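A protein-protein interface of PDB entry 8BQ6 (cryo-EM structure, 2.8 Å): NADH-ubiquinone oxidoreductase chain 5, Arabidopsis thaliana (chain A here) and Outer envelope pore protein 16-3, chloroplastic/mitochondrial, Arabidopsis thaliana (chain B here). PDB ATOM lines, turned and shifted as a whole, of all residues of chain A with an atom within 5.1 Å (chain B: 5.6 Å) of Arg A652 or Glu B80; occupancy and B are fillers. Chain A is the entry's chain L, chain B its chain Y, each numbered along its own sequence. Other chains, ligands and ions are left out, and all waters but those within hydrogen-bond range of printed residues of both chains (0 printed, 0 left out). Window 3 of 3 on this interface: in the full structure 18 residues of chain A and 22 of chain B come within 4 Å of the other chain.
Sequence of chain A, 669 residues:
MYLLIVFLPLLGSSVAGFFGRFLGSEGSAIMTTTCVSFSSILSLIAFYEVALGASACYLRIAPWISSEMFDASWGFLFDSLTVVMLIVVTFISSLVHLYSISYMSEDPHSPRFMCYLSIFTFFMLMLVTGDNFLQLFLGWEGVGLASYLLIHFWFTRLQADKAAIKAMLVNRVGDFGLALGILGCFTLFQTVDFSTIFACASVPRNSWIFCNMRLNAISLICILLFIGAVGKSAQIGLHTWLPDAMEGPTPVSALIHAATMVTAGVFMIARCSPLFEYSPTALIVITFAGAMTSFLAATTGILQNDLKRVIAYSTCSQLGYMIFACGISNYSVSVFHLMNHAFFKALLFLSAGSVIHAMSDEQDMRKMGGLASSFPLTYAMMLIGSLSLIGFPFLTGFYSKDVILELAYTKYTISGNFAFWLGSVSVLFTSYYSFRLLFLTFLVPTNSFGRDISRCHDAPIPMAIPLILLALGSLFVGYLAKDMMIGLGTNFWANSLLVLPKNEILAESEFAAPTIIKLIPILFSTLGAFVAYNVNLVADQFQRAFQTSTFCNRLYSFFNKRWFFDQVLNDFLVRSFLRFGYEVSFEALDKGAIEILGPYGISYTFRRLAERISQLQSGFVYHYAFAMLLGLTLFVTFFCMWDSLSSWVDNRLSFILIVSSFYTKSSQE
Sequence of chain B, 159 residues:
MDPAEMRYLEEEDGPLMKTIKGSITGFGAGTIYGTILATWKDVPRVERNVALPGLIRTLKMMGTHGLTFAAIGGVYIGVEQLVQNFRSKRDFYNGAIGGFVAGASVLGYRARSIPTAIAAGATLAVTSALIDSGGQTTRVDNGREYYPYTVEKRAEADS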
ATOM      1  N   ASP A 650      -8.699 -11.379   3.131  1.00  0.00           N
ATOM      2  CA  ASP A 650      -8.390 -10.429   2.076  1.00  0.00           C
ATOM      3  C   ASP A 650      -7.162 -10.926   1.328  1.00  0.00           C
ATOM      4  O   ASP A 650      -6.383 -11.728   1.851  1.00  0.00           O
ATOM      5  CB  ASP A 650      -8.142  -9.017   2.626  1.00  0.00           C
ATOM      6  CG  ASP A 650      -9.412  -8.354   3.131  1.00  0.00           C
ATOM      7  OD1 ASP A 650     -10.511  -8.850   2.805  1.00  0.00           O
ATOM      8  OD2 ASP A 650      -9.312  -7.343   3.858  1.00  0.00           O
ATOM      9  N   ASN A 651      -7.008 -10.464   0.085  1.00  0.00           N
ATOM     10  CA  ASN A 651      -5.815 -10.817  -0.677  1.00  0.00           C
ATOM     11  C   ASN A 651      -4.563 -10.183  -0.084  1.00  0.00           C
ATOM     12  O   ASN A 651      -3.507 -10.822  -0.057  1.00  0.00           O
ATOM     13  CB  ASN A 651      -5.987 -10.422  -2.143  1.00  0.00           C
ATOM     14  CG  ASN A 651      -6.646 -11.515  -2.968  1.00  0.00           C
ATOM     15  OD1 ASN A 651      -6.550 -12.698  -2.639  1.00  0.00           O
ATOM     16  ND2 ASN A 651      -7.326 -11.122  -4.040  1.00  0.00           N
ATOM     17  N   ARG A 652      -4.660  -8.947   0.414  1.00  0.00           N
ATOM     18  CA  ARG A 652      -3.507  -8.292   1.029  1.00  0.00           C
ATOM     19  C   ARG A 652      -2.930  -9.134   2.162  1.00  0.00           C
ATOM     20  O   ARG A 652      -1.726  -9.406   2.201  1.00  0.00           O
ATOM     21  CB  ARG A 652      -3.904  -6.911   1.551  1.00  0.00           C
ATOM     22  CG  ARG A 652      -4.899  -6.163   0.688  1.00  0.00           C
ATOM     23  CD  ARG A 652      -4.293  -4.882   0.148  1.00  0.00           C
ATOM     24  NE  ARG A 652      -3.565  -4.152   1.181  1.00  0.00           N
ATOM     25  CZ  ARG A 652      -4.123  -3.297   2.026  1.00  0.00           C
ATOM     26  NH1 ARG A 652      -5.425  -3.064   2.015  1.00  0.00           N
ATOM     27  NH2 ARG A 652      -3.356  -2.668   2.913  1.00  0.00           N
ATOM     28  N   LEU A 653      -3.789  -9.561   3.092  1.00  0.00           N
ATOM     29  CA  LEU A 653      -3.329 -10.318   4.252  1.00  0.00           C
ATOM     30  C   LEU A 653      -2.557 -11.562   3.827  1.00  0.00           C
ATOM     31  O   LEU A 653      -1.490 -11.862   4.377  1.00  0.00           O
ATOM     32  CB  LEU A 653      -4.514 -10.711   5.139  1.00  0.00           C
ATOM     33  CG  LEU A 653      -5.271  -9.561   5.806  1.00  0.00           C
ATOM     34  CD1 LEU A 653      -6.503 -10.080   6.532  1.00  0.00           C
ATOM     35  CD2 LEU A 653      -4.364  -8.799   6.759  1.00  0.00           C
ATOM     36  N   SER A 654      -3.066 -12.276   2.820  1.00  0.00           N
ATOM     37  CA  SER A 654      -2.504 -13.554   2.404  1.00  0.00           C
ATOM     38  C   SER A 654      -1.029 -13.444   2.030  1.00  0.00           C
ATOM     39  O   SER A 654      -0.183 -14.170   2.564  1.00  0.00           O
ATOM     40  CB  SER A 654      -3.319 -14.106   1.229  1.00  0.00           C
ATOM     41  OG  SER A 654      -2.521 -14.910   0.378  1.00  0.00           O
ATOM     42  N   PHE A 655      -0.706 -12.515   1.128  1.00  0.00           N
ATOM     43  CA  PHE A 655       0.685 -12.330   0.724  1.00  0.00           C
ATOM     44  C   PHE A 655       1.520 -11.762   1.862  1.00  0.00           C
ATOM     45  O   PHE A 655       2.716 -12.058   1.967  1.00  0.00           O
ATOM     46  CB  PHE A 655       0.764 -11.420  -0.500  1.00  0.00           C
ATOM     47  CG  PHE A 655      -0.180 -11.805  -1.594  1.00  0.00           C
ATOM     48  CD1 PHE A 655       0.027 -12.959  -2.327  1.00  0.00           C
ATOM     49  CD2 PHE A 655      -1.274 -11.015  -1.890  1.00  0.00           C
ATOM     50  CE1 PHE A 655      -0.842 -13.319  -3.333  1.00  0.00           C
ATOM     51  CE2 PHE A 655      -2.152 -11.371  -2.890  1.00  0.00           C
ATOM     52  CZ  PHE A 655      -1.934 -12.525  -3.615  1.00  0.00           C
ATOM     53  N   ILE A 656       0.915 -10.933   2.716  1.00  0.00           N
ATOM     54  CA  ILE A 656       1.636 -10.425   3.879  1.00  0.00           C
ATOM     55  C   ILE A 656       2.140 -11.584   4.730  1.00  0.00           C
ATOM     56  O   ILE A 656       3.310 -11.622   5.126  1.00  0.00           O
ATOM     57  CB  ILE A 656       0.747  -9.467   4.694  1.00  0.00           C
ATOM     58  CG1 ILE A 656       0.475  -8.172   3.920  1.00  0.00           C
ATOM     59  CG2 ILE A 656       1.376  -9.170   6.042  1.00  0.00           C
ATOM     60  CD1 ILE A 656       1.680  -7.611   3.180  1.00  0.00           C
ATOM     61  N   VAL B  75      -3.042  -6.638  13.629  1.00  0.00           N
ATOM     62  CA  VAL B  75      -2.433  -5.317  13.766  1.00  0.00           C
ATOM     63  C   VAL B  75      -2.285  -4.649  12.407  1.00  0.00           C
ATOM     64  O   VAL B  75      -2.469  -3.432  12.279  1.00  0.00           O
ATOM     65  CB  VAL B  75      -1.081  -5.425  14.496  1.00  0.00           C
ATOM     66  CG1 VAL B  75      -0.135  -4.323  14.050  1.00  0.00           C
ATOM     67  CG2 VAL B  75      -1.285  -5.368  15.995  1.00  0.00           C
ATOM     68  N   TYR B  76      -1.947  -5.426  11.374  1.00  0.00           N
ATOM     69  CA  TYR B  76      -1.794  -4.864  10.036  1.00  0.00           C
ATOM     70  C   TYR B  76      -3.023  -4.058   9.634  1.00  0.00           C
ATOM     71  O   TYR B  76      -2.946  -2.843   9.410  1.00  0.00           O
ATOM     72  CB  TYR B  76      -1.536  -5.997   9.045  1.00  0.00           C
ATOM     73  CG  TYR B  76      -1.531  -5.601   7.591  1.00  0.00           C
ATOM     74  CD1 TYR B  76      -2.239  -6.339   6.658  1.00  0.00           C
ATOM     75  CD2 TYR B  76      -0.804  -4.508   7.145  1.00  0.00           C
ATOM     76  CE1 TYR B  76      -2.236  -5.999   5.327  1.00  0.00           C
ATOM     77  CE2 TYR B  76      -0.794  -4.157   5.809  1.00  0.00           C
ATOM     78  CZ  TYR B  76      -1.514  -4.910   4.905  1.00  0.00           C
ATOM     79  OH  TYR B  76      -1.519  -4.581   3.571  1.00  0.00           O
ATOM     80  N   ILE B  77      -4.180  -4.717   9.573  1.00  0.00           N
ATOM     81  CA  ILE B  77      -5.386  -4.027   9.136  1.00  0.00           C
ATOM     82  C   ILE B  77      -5.863  -3.032  10.182  1.00  0.00           C
ATOM     83  O   ILE B  77      -6.441  -1.999   9.831  1.00  0.00           O
ATOM     84  CB  ILE B  77      -6.483  -5.039   8.775  1.00  0.00           C
ATOM     85  CG1 ILE B  77      -6.368  -6.272   9.658  1.00  0.00           C
ATOM     86  CG2 ILE B  77      -6.390  -5.427   7.312  1.00  0.00           C
ATOM     87  CD1 ILE B  77      -7.422  -7.270   9.370  1.00  0.00           C
ATOM     88  N   GLY B  78      -5.644  -3.305  11.470  1.00  0.00           N
ATOM     89  CA  GLY B  78      -6.052  -2.343  12.479  1.00  0.00           C
ATOM     90  C   GLY B  78      -5.374  -1.002  12.285  1.00  0.00           C
ATOM     91  O   GLY B  78      -6.030   0.042  12.237  1.00  0.00           O
ATOM     92  N   VAL B  79      -4.053  -1.021  12.117  1.00  0.00           N
ATOM     93  CA  VAL B  79      -3.319   0.215  11.882  1.00  0.00           C
ATOM     94  C   VAL B  79      -3.643   0.776  10.506  1.00  0.00           C
ATOM     95  O   VAL B  79      -3.666   1.997  10.312  1.00  0.00           O
ATOM     96  CB  VAL B  79      -1.812  -0.020  12.075  1.00  0.00           C
ATOM     97  CG1 VAL B  79      -1.016   1.175  11.583  1.00  0.00           C
ATOM     98  CG2 VAL B  79      -1.526  -0.266  13.540  1.00  0.00           C
ATOM     99  N   GLU B  80      -3.931  -0.093   9.534  1.00  0.00           N
ATOM    100  CA  GLU B  80      -4.313   0.407   8.219  1.00  0.00           C
ATOM    101  C   GLU B  80      -5.571   1.263   8.307  1.00  0.00           C
ATOM    102  O   GLU B  80      -5.625   2.366   7.752  1.00  0.00           O
ATOM    103  CB  GLU B  80      -4.522  -0.749   7.246  1.00  0.00           C
ATOM    104  CG  GLU B  80      -5.095  -0.298   5.916  1.00  0.00           C
ATOM    105  CD  GLU B  80      -5.668  -1.432   5.103  1.00  0.00           C
ATOM    106  OE1 GLU B  80      -5.425  -2.606   5.455  1.00  0.00           O
ATOM    107  OE2 GLU B  80      -6.348  -1.147   4.095  1.00  0.00           O
ATOM    108  N   GLN B  81      -6.588   0.780   9.022  1.00  0.00           N
ATOM    109  CA  GLN B  81      -7.822   1.553   9.136  1.00  0.00           C
ATOM    110  C   GLN B  81      -7.636   2.764  10.040  1.00  0.00           C
ATOM    111  O   GLN B  81      -8.107   3.860   9.715  1.00  0.00           O
ATOM    112  CB  GLN B  81      -8.968   0.674   9.635  1.00  0.00           C
ATOM    113  CG  GLN B  81      -9.001  -0.708   9.011  1.00  0.00           C
ATOM    114  CD  GLN B  81      -9.578  -0.702   7.616  1.00  0.00           C
ATOM    115  OE1 GLN B  81     -10.079   0.316   7.144  1.00  0.00           O
ATOM    116  NE2 GLN B  81      -9.511  -1.846   6.944  1.00  0.00           N
ATOM    117  N   LEU B  82      -6.932   2.602  11.162  1.00  0.00           N
ATOM    118  CA  LEU B  82      -6.678   3.728  12.052  1.00  0.00           C
ATOM    119  C   LEU B  82      -5.819   4.802  11.400  1.00  0.00           C
ATOM    120  O   LEU B  82      -5.756   5.923  11.914  1.00  0.00           O
ATOM    121  CB  LEU B  82      -6.009   3.233  13.328  1.00  0.00           C
ATOM    122  CG  LEU B  82      -6.933   2.395  14.207  1.00  0.00           C
ATOM    123  CD1 LEU B  82      -6.104   1.558  15.165  1.00  0.00           C
ATOM    124  CD2 LEU B  82      -7.938   3.264  14.955  1.00  0.00           C
ATOM    125  N   VAL B  83      -5.139   4.478  10.308  1.00  0.00           N
ATOM    126  CA  VAL B  83      -4.505   5.494   9.482  1.00  0.00           C
ATOM    127  C   VAL B  83      -5.515   6.130   8.537  1.00  0.00           C
ATOM    128  O   VAL B  83      -5.644   7.355   8.485  1.00  0.00           O
ATOM    129  CB  VAL B  83      -3.323   4.877   8.710  1.00  0.00           C
ATOM    130  CG1 VAL B  83      -3.030   5.678   7.460  1.00  0.00           C
ATOM    131  CG2 VAL B  83      -2.089   4.803   9.594  1.00  0.00           C
ATOM    132  N   GLN B  84      -6.254   5.305   7.800  1.00  0.00           N
ATOM    133  CA  GLN B  84      -7.219   5.783   6.820  1.00  0.00           C
ATOM    134  C   GLN B  84      -8.493   6.321   7.461  1.00  0.00           C
ATOM    135  O   GLN B  84      -9.305   6.944   6.771  1.00  0.00           O
ATOM    136  CB  GLN B  84      -7.541   4.652   5.841  1.00  0.00           C
ATOM    137  CG  GLN B  84      -8.418   5.034   4.668  1.00  0.00           C
ATOM    138  CD  GLN B  84      -9.804   4.463   4.818  1.00  0.00           C
ATOM    139  OE1 GLN B  84     -10.208   4.087   5.917  1.00  0.00           O
ATOM    140  NE2 GLN B  84     -10.537   4.378   3.719  1.00  0.00           N
ATOM    141  N   ASN B  85      -8.694   6.102   8.757  1.00  0.00           N
ATOM    142  CA  ASN B  85      -9.825   6.712   9.441  1.00  0.00           C
ATOM    143  C   ASN B  85      -9.511   8.145   9.867  1.00  0.00           C
ATOM    144  O   ASN B  85     -10.247   9.072   9.517  1.00  0.00           O
ATOM    145  CB  ASN B  85     -10.228   5.852  10.644  1.00  0.00           C
ATOM    146  CG  ASN B  85     -11.396   6.423  11.406  1.00  0.00           C
ATOM    147  OD1 ASN B  85     -12.532   6.407  10.931  1.00  0.00           O
ATOM    148  ND2 ASN B  85     -11.132   6.907  12.614  1.00  0.00           N
ATOM    149  N   ASN B  94      -1.543   4.648   2.982  1.00  0.00           N
ATOM    150  CA  ASN B  94      -2.324   4.074   4.106  1.00  0.00           C
ATOM    151  C   ASN B  94      -2.189   2.556   3.926  1.00  0.00           C
ATOM    152  O   ASN B  94      -2.545   2.048   2.841  1.00  0.00           O
ATOM    153  CB  ASN B  94      -3.751   4.635   4.172  1.00  0.00           C
ATOM    154  CG  ASN B  94      -4.644   4.316   2.990  1.00  0.00           C
ATOM    155  OD1 ASN B  94      -4.539   3.245   2.400  1.00  0.00           O
ATOM    156  ND2 ASN B  94      -5.511   5.244   2.621  1.00  0.00           N
ATOM    157  N   GLY B  95      -1.618   1.869   4.910  1.00  0.00           N
ATOM    158  CA  GLY B  95      -1.380   0.427   4.720  1.00  0.00           C
ATOM    159  C   GLY B  95       0.103   0.111   4.700  1.00  0.00           C
ATOM    160  O   GLY B  95       0.481  -0.900   5.316  1.00  0.00           O
ATOM    161  N   GLY B  98       0.751   0.247   8.139  1.00  0.00           N
ATOM    162  CA  GLY B  98       0.251  -0.909   8.869  1.00  0.00           C
ATOM    163  C   GLY B  98       1.121  -2.139   8.697  1.00  0.00           C
ATOM    164  O   GLY B  98       1.419  -2.844   9.665  1.00  0.00           O
ATOM    165  N   SER B 128       2.975  -4.731   0.819  1.00  0.00           N
ATOM    166  CA  SER B 128       1.685  -4.055   0.822  1.00  0.00           C
ATOM    167  C   SER B 128       1.661  -2.858  -0.118  1.00  0.00           C
ATOM    168  O   SER B 128       0.576  -2.401  -0.493  1.00  0.00           O
ATOM    169  CB  SER B 128       1.329  -3.617   2.241  1.00  0.00           C
ATOM    170  OG  SER B 128       2.130  -2.520   2.645  1.00  0.00           O
ATOM    171  N   ILE B 131       0.476  -3.712  -3.705  1.00  0.00           N
ATOM    172  CA  ILE B 131      -0.942  -4.039  -3.825  1.00  0.00           C
ATOM    173  C   ILE B 131      -1.815  -2.809  -3.596  1.00  0.00           C
ATOM    174  O   ILE B 131      -2.391  -2.257  -4.536  1.00  0.00           O
ATOM    175  CB  ILE B 131      -1.330  -5.164  -2.845  1.00  0.00           C
ATOM    176  CG1 ILE B 131      -0.319  -6.309  -2.922  1.00  0.00           C
ATOM    177  CG2 ILE B 131      -2.726  -5.682  -3.153  1.00  0.00           C
ATOM    178  CD1 ILE B 131      -0.700  -7.518  -2.097  1.00  0.00           C
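OH of Tyr B76 sits at hydrogen-bond distance from NH2 of Arg A652, 2.7 Å away. NH1 of Arg A652 is in salt-bridge range of OE2 of Glu B80 (3.0 Å).
Of the 16 printed residues of chain B, 5 touch a printed residue of chain A.
Arg A652 touches just these residues of chain B: Tyr B76 (2.7 Å), Glu B80 (3.0 Å) and Ile B131 (3.7 Å). Printed residues of chain A within 4 Å of Glu B80: Arg A652 (3.0 Å). Of the printed residues of chain B, Phe A655 touches Ile B131 (3.5 Å). Of the printed residues of chain A, Ser B128 touches Ile A656 (3.9 Å). Of the printed residues of chain B, Leu A653 touches Tyr B76 (3.3 Å) and Ile B77 (3.97 Å). Of the printed residues of chain A, Ile B77 touches Leu A653. Printed residues of chain A within 4 Å of Ile B131: Arg A652 (3.7 Å) and Phe A655 (3.5 Å). The nearest residue of chain B that does not touch Arg A652 is Gly B95 (4.1 Å). The nearest printed residue of chain B that does not touch Phe A655 is Ser B128 (7.2 Å).
Arg A652 touches Ile B131 (CD to CG2, 3.7 Å). Leu A653 touches Tyr B76. Ile B77 touches Leu A653. CD2 of Phe A655 touches CD1 of Ile B131 (3.5 Å). Tyr B76 touches Ile A656 (CE1 to CG1, 3.7 Å). Ile A656 touches Ser B128.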
